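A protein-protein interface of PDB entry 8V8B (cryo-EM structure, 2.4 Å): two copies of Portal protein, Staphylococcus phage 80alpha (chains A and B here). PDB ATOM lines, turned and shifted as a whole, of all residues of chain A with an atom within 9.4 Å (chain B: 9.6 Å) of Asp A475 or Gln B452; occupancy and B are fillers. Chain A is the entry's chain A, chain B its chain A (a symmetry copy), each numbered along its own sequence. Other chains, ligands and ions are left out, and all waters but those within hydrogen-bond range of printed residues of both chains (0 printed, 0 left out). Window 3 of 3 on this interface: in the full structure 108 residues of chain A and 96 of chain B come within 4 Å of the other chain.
OE2 of Glu A468 lies within hydrogen-bond range of OG of Ser B451 (2.8 Å).
The side-chain hydroxyl (OG1) of Thr B454 sits at hydrogen-bond distance from the side-chain carboxylate (OE1) of Glu A468, 2.8 Å away.
N of Gln B452 sits at hydrogen-bond distance from OD2 of Asp A475.
The side-chain carboxylate (OE1) of Glu A474 is in salt-bridge range of the side-chain amino group (NZ) of Lys A471 (2.9 Å).
OG of Ser B451 sits at hydrogen-bond distance from OG1 of Thr B454, 3.3 Å away.
The backbone carbonyl oxygen (O) of Thr B454 sits at hydrogen-bond distance from the side-chain hydroxyl (OG) of Ser B457 (2.6 Å).
Ile B450 touches Glu A468 (CG2 to OE2, 3.6 Å).
Lys A471 touches Ser B451 (CB to CB, 3.8 Å).
CD1 of Ile A472 touches O of Lys B449, 3.6 Å away.
Ile A472 touches Ser B451.
Ser B451 touches Asp A475 (CA to OD2, 3.1 Å).
Printed residues of chain B within 4 Å of Glu A468: Ile B450, Ser B451 and Thr B454.
Of the printed residues of chain B, Lys A471 touches Ser B451 (3.8 Å).
Asp A475 touches two residues of chain B.
Printed residues of chain A within 4 Å of Ile B450: Glu A468.
Ser B451 touches four residues of chain A.
Of chain A, only Asp A475 comes within 4 Å of Gln B452.
Printed residues of chain A within 4 Å of Thr B454: Glu A468 (2.8 Å).
Glu B468 touches none of the printed residues of chain A.
The nearest residue of chain A that does not touch Gln B452 is Glu A468 (5.8 Å).
The nearest printed residue of chain A that does not touch Ile B450 is Ile A472 (4.2 Å).
Of the 10 printed residues of chain A, 4 touch a printed residue of chain B.
Hydrophobic or aromatic side chains of chain A within 4 Å of the printed part of chain B: Ile A472.
Of the 20 printed residues of chain B, 5 touch a printed residue of chain A.
Along chain B the printed residues that touch a printed residue of chain A span positions 449 to 454.
Among the printed residues, 8 pairs touch across the chains.
6 positions are printed for both chains.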
ATOM      1  N   LEU A 467      -9.375  18.982  21.950  1.00  0.00           N
ATOM      2  CA  LEU A 467     -10.285  18.715  20.843  1.00  0.00           C
ATOM      3  C   LEU A 467      -9.693  17.739  19.831  1.00  0.00           C
ATOM      4  O   LEU A 467     -10.440  17.026  19.145  1.00  0.00           O
ATOM      5  CB  LEU A 467     -10.650  20.032  20.159  1.00  0.00           C
ATOM      6  CG  LEU A 467     -11.221  21.103  21.094  1.00  0.00           C
ATOM      7  CD1 LEU A 467     -11.586  22.360  20.310  1.00  0.00           C
ATOM      8  CD2 LEU A 467     -12.434  20.581  21.866  1.00  0.00           C
ATOM      9  N   GLU A 468      -8.364  17.713  19.712  1.00  0.00           N
ATOM     10  CA  GLU A 468      -7.730  16.981  18.621  1.00  0.00           C
ATOM     11  C   GLU A 468      -7.942  15.476  18.742  1.00  0.00           C
ATOM     12  O   GLU A 468      -8.115  14.795  17.728  1.00  0.00           O
ATOM     13  CB  GLU A 468      -6.238  17.307  18.573  1.00  0.00           C
ATOM     14  CG  GLU A 468      -5.534  16.786  17.325  1.00  0.00           C
ATOM     15  CD  GLU A 468      -6.098  17.379  16.049  1.00  0.00           C
ATOM     16  OE1 GLU A 468      -6.673  18.484  16.115  1.00  0.00           O
ATOM     17  OE2 GLU A 468      -5.973  16.742  14.983  1.00  0.00           O
ATOM     18  N   VAL A 469      -7.887  14.926  19.955  1.00  0.00           N
ATOM     19  CA  VAL A 469      -8.115  13.489  20.116  1.00  0.00           C
ATOM     20  C   VAL A 469      -9.513  13.110  19.634  1.00  0.00           C
ATOM     21  O   VAL A 469      -9.711  12.072  18.982  1.00  0.00           O
ATOM     22  CB  VAL A 469      -7.890  13.077  21.584  1.00  0.00           C
ATOM     23  CG1 VAL A 469      -8.064  11.575  21.753  1.00  0.00           C
ATOM     24  CG2 VAL A 469      -6.503  13.510  22.054  1.00  0.00           C
ATOM     25  N   LYS A 470     -10.498  13.964  19.914  1.00  0.00           N
ATOM     26  CA  LYS A 470     -11.854  13.713  19.437  1.00  0.00           C
ATOM     27  C   LYS A 470     -11.922  13.785  17.920  1.00  0.00           C
ATOM     28  O   LYS A 470     -12.498  12.906  17.275  1.00  0.00           O
ATOM     29  CB  LYS A 470     -12.829  14.704  20.069  1.00  0.00           C
ATOM     30  CG  LYS A 470     -12.654  14.863  21.572  1.00  0.00           C
ATOM     31  CD  LYS A 470     -13.737  15.746  22.173  1.00  0.00           C
ATOM     32  CE  LYS A 470     -13.297  16.311  23.514  1.00  0.00           C
ATOM     33  NZ  LYS A 470     -12.999  15.237  24.506  1.00  0.00           N
ATOM     34  N   LYS A 471     -11.345  14.834  17.330  1.00  0.00           N
ATOM     35  CA  LYS A 471     -11.326  14.923  15.871  1.00  0.00           C
ATOM     36  C   LYS A 471     -10.606  13.739  15.234  1.00  0.00           C
ATOM     37  O   LYS A 471     -10.962  13.319  14.127  1.00  0.00           O
ATOM     38  CB  LYS A 471     -10.669  16.232  15.435  1.00  0.00           C
ATOM     39  CG  LYS A 471     -11.515  17.458  15.711  1.00  0.00           C
ATOM     40  CD  LYS A 471     -12.550  17.651  14.617  1.00  0.00           C
ATOM     41  CE  LYS A 471     -13.648  18.610  15.046  1.00  0.00           C
ATOM     42  NZ  LYS A 471     -14.624  17.953  15.962  1.00  0.00           N
ATOM     43  N   ILE A 472      -9.599  13.190  15.911  1.00  0.00           N
ATOM     44  CA  ILE A 472      -8.905  12.010  15.402  1.00  0.00           C
ATOM     45  C   ILE A 472      -9.825  10.798  15.412  1.00  0.00           C
ATOM     46  O   ILE A 472      -9.906  10.053  14.428  1.00  0.00           O
ATOM     47  CB  ILE A 472      -7.626  11.746  16.217  1.00  0.00           C
ATOM     48  CG1 ILE A 472      -6.569  12.803  15.902  1.00  0.00           C
ATOM     49  CG2 ILE A 472      -7.086  10.351  15.929  1.00  0.00           C
ATOM     50  CD1 ILE A 472      -5.518  12.938  16.974  1.00  0.00           C
ATOM     51  N   GLU A 473     -10.532  10.579  16.523  1.00  0.00           N
ATOM     52  CA  GLU A 473     -11.487   9.474  16.559  1.00  0.00           C
ATOM     53  C   GLU A 473     -12.601   9.667  15.538  1.00  0.00           C
ATOM     54  O   GLU A 473     -13.110   8.688  14.979  1.00  0.00           O
ATOM     55  CB  GLU A 473     -12.072   9.323  17.962  1.00  0.00           C
ATOM     56  CG  GLU A 473     -11.056   8.866  19.001  1.00  0.00           C
ATOM     57  CD  GLU A 473     -11.677   8.650  20.367  1.00  0.00           C
ATOM     58  OE1 GLU A 473     -12.538   7.754  20.497  1.00  0.00           O
ATOM     59  OE2 GLU A 473     -11.309   9.384  21.306  1.00  0.00           O
ATOM     60  N   GLU A 474     -12.989  10.915  15.282  1.00  0.00           N
ATOM     61  CA  GLU A 474     -13.947  11.217  14.227  1.00  0.00           C
ATOM     62  C   GLU A 474     -13.411  10.879  12.843  1.00  0.00           C
ATOM     63  O   GLU A 474     -14.204  10.686  11.916  1.00  0.00           O
ATOM     64  CB  GLU A 474     -14.321  12.698  14.276  1.00  0.00           C
ATOM     65  CG  GLU A 474     -15.101  13.115  15.513  1.00  0.00           C
ATOM     66  CD  GLU A 474     -15.060  14.617  15.738  1.00  0.00           C
ATOM     67  OE1 GLU A 474     -15.155  15.369  14.744  1.00  0.00           O
ATOM     68  OE2 GLU A 474     -14.934  15.048  16.903  1.00  0.00           O
ATOM     69  N   ASP A 475     -12.093  10.816  12.677  1.00  0.00           N
ATOM     70  CA  ASP A 475     -11.491  10.301  11.454  1.00  0.00           C
ATOM     71  C   ASP A 475     -11.286   8.793  11.486  1.00  0.00           C
ATOM     72  O   ASP A 475     -10.720   8.240  10.538  1.00  0.00           O
ATOM     73  CB  ASP A 475     -10.149  10.994  11.189  1.00  0.00           C
ATOM     74  CG  ASP A 475     -10.307  12.465  10.851  1.00  0.00           C
ATOM     75  OD1 ASP A 475     -11.434  12.885  10.511  1.00  0.00           O
ATOM     76  OD2 ASP A 475      -9.304  13.204  10.922  1.00  0.00           O
ATOM     77  N   GLU A 476     -11.725   8.120  12.546  1.00  0.00           N
ATOM     78  CA  GLU A 476     -11.573   6.675  12.645  1.00  0.00           C
ATOM     79  C   GLU A 476     -12.847   6.044  13.200  1.00  0.00           C
ATOM     80  O   GLU A 476     -13.301   5.003  12.721  1.00  0.00           O
ATOM     81  CB  GLU A 476     -10.380   6.318  13.534  1.00  0.00           C
ATOM     82  CG  GLU A 476     -10.124   4.823  13.642  1.00  0.00           C
ATOM     83  CD  GLU A 476      -8.899   4.493  14.469  1.00  0.00           C
ATOM     84  OE1 GLU A 476      -8.559   5.285  15.372  1.00  0.00           O
ATOM     85  OE2 GLU A 476      -8.283   3.435  14.226  1.00  0.00           O
ATOM     86  N   LYS B 449      -0.486  11.549  15.772  1.00  0.00           N
ATOM     87  CA  LYS B 449      -1.559  11.569  14.791  1.00  0.00           C
ATOM     88  C   LYS B 449      -2.183  12.957  14.722  1.00  0.00           C
ATOM     89  O   LYS B 449      -2.184  13.706  15.704  1.00  0.00           O
ATOM     90  CB  LYS B 449      -2.638  10.526  15.119  1.00  0.00           C
ATOM     91  CG  LYS B 449      -2.259   9.103  14.721  1.00  0.00           C
ATOM     92  CD  LYS B 449      -3.428   8.146  14.916  1.00  0.00           C
ATOM     93  CE  LYS B 449      -3.172   6.794  14.259  1.00  0.00           C
ATOM     94  NZ  LYS B 449      -2.098   6.020  14.942  1.00  0.00           N
ATOM     95  N   ILE B 450      -2.714  13.296  13.550  1.00  0.00           N
ATOM     96  CA  ILE B 450      -3.430  14.553  13.343  1.00  0.00           C
ATOM     97  C   ILE B 450      -4.673  14.272  12.513  1.00  0.00           C
ATOM     98  O   ILE B 450      -4.641  13.460  11.584  1.00  0.00           O
ATOM     99  CB  ILE B 450      -2.545  15.615  12.656  1.00  0.00           C
ATOM    100  CG1 ILE B 450      -1.154  15.640  13.282  1.00  0.00           C
ATOM    101  CG2 ILE B 450      -3.177  16.997  12.766  1.00  0.00           C
ATOM    102  CD1 ILE B 450      -0.247  16.676  12.675  1.00  0.00           C
ATOM    103  N   SER B 451      -5.769  14.939  12.853  1.00  0.00           N
ATOM    104  CA  SER B 451      -6.957  14.900  12.015  1.00  0.00           C
ATOM    105  C   SER B 451      -6.696  15.587  10.679  1.00  0.00           C
ATOM    106  O   SER B 451      -5.865  16.493  10.571  1.00  0.00           O
ATOM    107  CB  SER B 451      -8.128  15.576  12.725  1.00  0.00           C
ATOM    108  OG  SER B 451      -7.858  16.948  12.947  1.00  0.00           O
ATOM    109  N   GLN B 452      -7.424  15.148   9.650  1.00  0.00           N
ATOM    110  CA  GLN B 452      -7.320  15.798   8.348  1.00  0.00           C
ATOM    111  C   GLN B 452      -7.629  17.288   8.447  1.00  0.00           C
ATOM    112  O   GLN B 452      -6.957  18.110   7.822  1.00  0.00           O
ATOM    113  CB  GLN B 452      -8.260  15.134   7.341  1.00  0.00           C
ATOM    114  CG  GLN B 452      -8.169  13.615   7.253  1.00  0.00           C
ATOM    115  CD  GLN B 452      -6.748  13.107   7.074  1.00  0.00           C
ATOM    116  OE1 GLN B 452      -6.025  13.551   6.181  1.00  0.00           O
ATOM    117  NE2 GLN B 452      -6.346  12.162   7.915  1.00  0.00           N
ATOM    118  N   THR B 453      -8.659  17.649   9.212  1.00  0.00           N
ATOM    119  CA  THR B 453      -9.053  19.052   9.339  1.00  0.00           C
ATOM    120  C   THR B 453      -7.912  19.924   9.865  1.00  0.00           C
ATOM    121  O   THR B 453      -7.607  20.982   9.302  1.00  0.00           O
ATOM    122  CB  THR B 453     -10.271  19.146  10.259  1.00  0.00           C
ATOM    123  OG1 THR B 453     -11.215  18.130   9.899  1.00  0.00           O
ATOM    124  CG2 THR B 453     -10.940  20.504  10.141  1.00  0.00           C
ATOM    125  N   THR B 454      -7.227  19.468  10.916  1.00  0.00           N
ATOM    126  CA  THR B 454      -6.152  20.273  11.492  1.00  0.00           C
ATOM    127  C   THR B 454      -4.919  20.281  10.596  1.00  0.00           C
ATOM    128  O   THR B 454      -4.267  21.324  10.425  1.00  0.00           O
ATOM    129  CB  THR B 454      -5.805  19.735  12.882  1.00  0.00           C
ATOM    130  OG1 THR B 454      -6.894  19.987  13.778  1.00  0.00           O
ATOM    131  CG2 THR B 454      -4.544  20.382  13.429  1.00  0.00           C
ATOM    132  N   LEU B 455      -4.601  19.139   9.992  1.00  0.00           N
ATOM    133  CA  LEU B 455      -3.484  19.101   9.063  1.00  0.00           C
ATOM    134  C   LEU B 455      -3.717  20.070   7.911  1.00  0.00           C
ATOM    135  O   LEU B 455      -2.806  20.801   7.508  1.00  0.00           O
ATOM    136  CB  LEU B 455      -3.291  17.673   8.553  1.00  0.00           C
ATOM    137  CG  LEU B 455      -2.084  17.413   7.655  1.00  0.00           C
ATOM    138  CD1 LEU B 455      -0.795  17.581   8.435  1.00  0.00           C
ATOM    139  CD2 LEU B 455      -2.164  16.017   7.050  1.00  0.00           C
ATOM    140  N   MET B 456      -4.939  20.094   7.377  1.00  0.00           N
ATOM    141  CA  MET B 456      -5.293  21.053   6.340  1.00  0.00           C
ATOM    142  C   MET B 456      -5.344  22.481   6.858  1.00  0.00           C
ATOM    143  O   MET B 456      -5.278  23.415   6.055  1.00  0.00           O
ATOM    144  CB  MET B 456      -6.645  20.689   5.735  1.00  0.00           C
ATOM    145  CG  MET B 456      -6.619  19.426   4.912  1.00  0.00           C
ATOM    146  SD  MET B 456      -8.269  18.916   4.410  1.00  0.00           S
ATOM    147  CE  MET B 456      -7.886  17.421   3.510  1.00  0.00           C
ATOM    148  N   SER B 457      -5.463  22.677   8.170  1.00  0.00           N
ATOM    149  CA  SER B 457      -5.398  24.036   8.687  1.00  0.00           C
ATOM    150  C   SER B 457      -3.967  24.505   8.910  1.00  0.00           C
ATOM    151  O   SER B 457      -3.750  25.706   9.102  1.00  0.00           O
ATOM    152  CB  SER B 457      -6.176  24.149  10.001  1.00  0.00           C
ATOM    153  OG  SER B 457      -5.475  23.524  11.062  1.00  0.00           O
ATOM    154  N   LEU B 458      -2.990  23.598   8.883  1.00  0.00           N
ATOM    155  CA  LEU B 458      -1.597  24.043   8.908  1.00  0.00           C
ATOM    156  C   LEU B 458      -1.112  24.551   7.550  1.00  0.00           C
ATOM    157  O   LEU B 458      -0.179  25.360   7.502  1.00  0.00           O
ATOM    158  CB  LEU B 458      -0.676  22.921   9.388  1.00  0.00           C
ATOM    159  CG  LEU B 458      -1.011  22.270  10.728  1.00  0.00           C
ATOM    160  CD1 LEU B 458       0.075  21.280  11.095  1.00  0.00           C
ATOM    161  CD2 LEU B 458      -1.184  23.304  11.827  1.00  0.00           C
ATOM    162  N   PHE B 459      -1.704  24.097   6.448  1.00  0.00           N
ATOM    163  CA  PHE B 459      -1.237  24.433   5.104  1.00  0.00           C
ATOM    164  C   PHE B 459      -2.269  25.307   4.401  1.00  0.00           C
ATOM    165  O   PHE B 459      -3.439  24.927   4.288  1.00  0.00           O
ATOM    166  CB  PHE B 459      -0.958  23.165   4.298  1.00  0.00           C
ATOM    167  CG  PHE B 459       0.164  22.335   4.855  1.00  0.00           C
ATOM    168  CD1 PHE B 459      -0.081  21.362   5.803  1.00  0.00           C
ATOM    169  CD2 PHE B 459       1.466  22.540   4.435  1.00  0.00           C
ATOM    170  CE1 PHE B 459       0.951  20.602   6.319  1.00  0.00           C
ATOM    171  CE2 PHE B 459       2.501  21.784   4.947  1.00  0.00           C
ATOM    172  CZ  PHE B 459       2.241  20.811   5.891  1.00  0.00           C
ATOM    173  N   PHE B 462      -5.081  25.019   0.980  1.00  0.00           N
ATOM    174  CA  PHE B 462      -6.490  24.631   1.083  1.00  0.00           C
ATOM    175  C   PHE B 462      -7.340  25.887   1.233  1.00  0.00           C
ATOM    176  O   PHE B 462      -7.431  26.471   2.314  1.00  0.00           O
ATOM    177  CB  PHE B 462      -6.697  23.661   2.238  1.00  0.00           C
ATOM    178  CG  PHE B 462      -5.993  22.352   2.048  1.00  0.00           C
ATOM    179  CD1 PHE B 462      -6.551  21.373   1.240  1.00  0.00           C
ATOM    180  CD2 PHE B 462      -4.758  22.114   2.625  1.00  0.00           C
ATOM    181  CE1 PHE B 462      -5.911  20.170   1.039  1.00  0.00           C
ATOM    182  CE2 PHE B 462      -4.113  20.915   2.429  1.00  0.00           C
ATOM    183  CZ  PHE B 462      -4.692  19.937   1.633  1.00  0.00           C
ATOM    184  N   PRO B 465     -11.039  24.347   3.584  1.00  0.00           N
ATOM    185  CA  PRO B 465     -10.845  22.903   3.804  1.00  0.00           C
ATOM    186  C   PRO B 465     -12.079  22.161   4.301  1.00  0.00           C
ATOM    187  O   PRO B 465     -12.105  20.928   4.207  1.00  0.00           O
ATOM    188  CB  PRO B 465      -9.723  22.860   4.852  1.00  0.00           C
ATOM    189  CG  PRO B 465      -9.848  24.156   5.578  1.00  0.00           C
ATOM    190  CD  PRO B 465     -10.286  25.157   4.556  1.00  0.00           C
ATOM    191  N   GLU B 466     -13.096  22.850   4.821  1.00  0.00           N
ATOM    192  CA  GLU B 466     -14.326  22.161   5.210  1.00  0.00           C
ATOM    193  C   GLU B 466     -14.971  21.446   4.029  1.00  0.00           C
ATOM    194  O   GLU B 466     -15.676  20.447   4.216  1.00  0.00           O
ATOM    195  CB  GLU B 466     -15.304  23.159   5.836  1.00  0.00           C
ATOM    196  CG  GLU B 466     -16.702  22.605   6.101  1.00  0.00           C
ATOM    197  CD  GLU B 466     -16.696  21.379   6.993  1.00  0.00           C
ATOM    198  OE1 GLU B 466     -15.758  21.235   7.809  1.00  0.00           O
ATOM    199  OE2 GLU B 466     -17.631  20.560   6.879  1.00  0.00           O
ATOM    200  N   GLU B 468     -13.052  20.141   1.578  1.00  0.00           N
ATOM    201  CA  GLU B 468     -12.096  19.170   1.056  1.00  0.00           C
ATOM    202  C   GLU B 468     -12.367  17.763   1.578  1.00  0.00           C
ATOM    203  O   GLU B 468     -12.194  16.789   0.842  1.00  0.00           O
ATOM    204  CB  GLU B 468     -10.672  19.602   1.406  1.00  0.00           C
ATOM    205  CG  GLU B 468      -9.592  18.788   0.702  1.00  0.00           C
ATOM    206  CD  GLU B 468      -9.669  18.903  -0.807  1.00  0.00           C
ATOM    207  OE1 GLU B 468     -10.209  19.915  -1.296  1.00  0.00           O
ATOM    208  OE2 GLU B 468      -9.197  17.982  -1.505  1.00  0.00           O
ATOM    209  N   VAL B 469     -12.746  17.623   2.849  1.00  0.00           N
ATOM    210  CA  VAL B 469     -13.044  16.292   3.379  1.00  0.00           C
ATOM    211  C   VAL B 469     -14.197  15.654   2.608  1.00  0.00           C
ATOM    212  O   VAL B 469     -14.180  14.451   2.300  1.00  0.00           O
ATOM    213  CB  VAL B 469     -13.348  16.377   4.888  1.00  0.00           C
ATOM    214  CG1 VAL B 469     -13.601  14.991   5.463  1.00  0.00           C
ATOM    215  CG2 VAL B 469     -12.200  17.060   5.626  1.00  0.00           C
ATOM    216  N   LYS B 470     -15.202  16.457   2.254  1.00  0.00           N
ATOM    217  CA  LYS B 470     -16.315  15.946   1.461  1.00  0.00           C
ATOM    218  C   LYS B 470     -15.853  15.538   0.071  1.00  0.00           C
ATOM    219  O   LYS B 470     -16.189  14.453  -0.410  1.00  0.00           O
ATOM    220  CB  LYS B 470     -17.428  16.989   1.377  1.00  0.00           C
ATOM    221  CG  LYS B 470     -17.778  17.621   2.716  1.00  0.00           C
ATOM    222  CD  LYS B 470     -18.983  18.541   2.603  1.00  0.00           C
ATOM    223  CE  LYS B 470     -19.021  19.531   3.755  1.00  0.00           C
ATOM    224  NZ  LYS B 470     -19.107  18.850   5.079  1.00  0.00           N
ATOM    225  N   ILE B 472     -12.992  14.570  -0.744  1.00  0.00           N
ATOM    226  CA  ILE B 472     -12.190  13.360  -0.584  1.00  0.00           C
ATOM    227  C   ILE B 472     -13.081  12.131  -0.491  1.00  0.00           C
ATOM    228  O   ILE B 472     -12.833  11.114  -1.149  1.00  0.00           O
ATOM    229  CB  ILE B 472     -11.276  13.481   0.648  1.00  0.00           C
ATOM    230  CG1 ILE B 472     -10.155  14.483   0.381  1.00  0.00           C
ATOM    231  CG2 ILE B 472     -10.698  12.122   1.023  1.00  0.00           C
ATOM    232  CD1 ILE B 472      -9.535  15.040   1.638  1.00  0.00           C
ATOM    233  N   GLU B 473     -14.133  12.202   0.329  1.00  0.00           N
ATOM    234  CA  GLU B 473     -15.064  11.078   0.400  1.00  0.00           C
ATOM    235  C   GLU B 473     -15.753  10.841  -0.940  1.00  0.00           C
ATOM    236  O   GLU B 473     -16.057   9.693  -1.288  1.00  0.00           O
ATOM    237  CB  GLU B 473     -16.100  11.315   1.496  1.00  0.00           C
ATOM    238  CG  GLU B 473     -15.514  11.298   2.903  1.00  0.00           C
ATOM    239  CD  GLU B 473     -16.573  11.458   3.975  1.00  0.00           C
ATOM    240  OE1 GLU B 473     -17.444  10.570   4.093  1.00  0.00           O
ATOM    241  OE2 GLU B 473     -16.537  12.478   4.694  1.00  0.00           O
ATOM    242  N   GLU B 476     -13.930   8.533  -2.800  1.00  0.00           N
ATOM    243  CA  GLU B 476     -13.852   7.210  -2.196  1.00  0.00           C
ATOM    244  C   GLU B 476     -15.252   6.666  -1.924  1.00  0.00           C
ATOM    245  O   GLU B 476     -15.533   5.491  -2.164  1.00  0.00           O
ATOM    246  CB  GLU B 476     -13.045   7.258  -0.896  1.00  0.00           C
ATOM    247  CG  GLU B 476     -12.873   5.900  -0.233  1.00  0.00           C
ATOM    248  CD  GLU B 476     -12.017   5.958   1.014  1.00  0.00           C
ATOM    249  OE1 GLU B 476     -11.992   7.019   1.672  1.00  0.00           O
ATOM    250  OE2 GLU B 476     -11.376   4.939   1.346  1.00  0.00           O
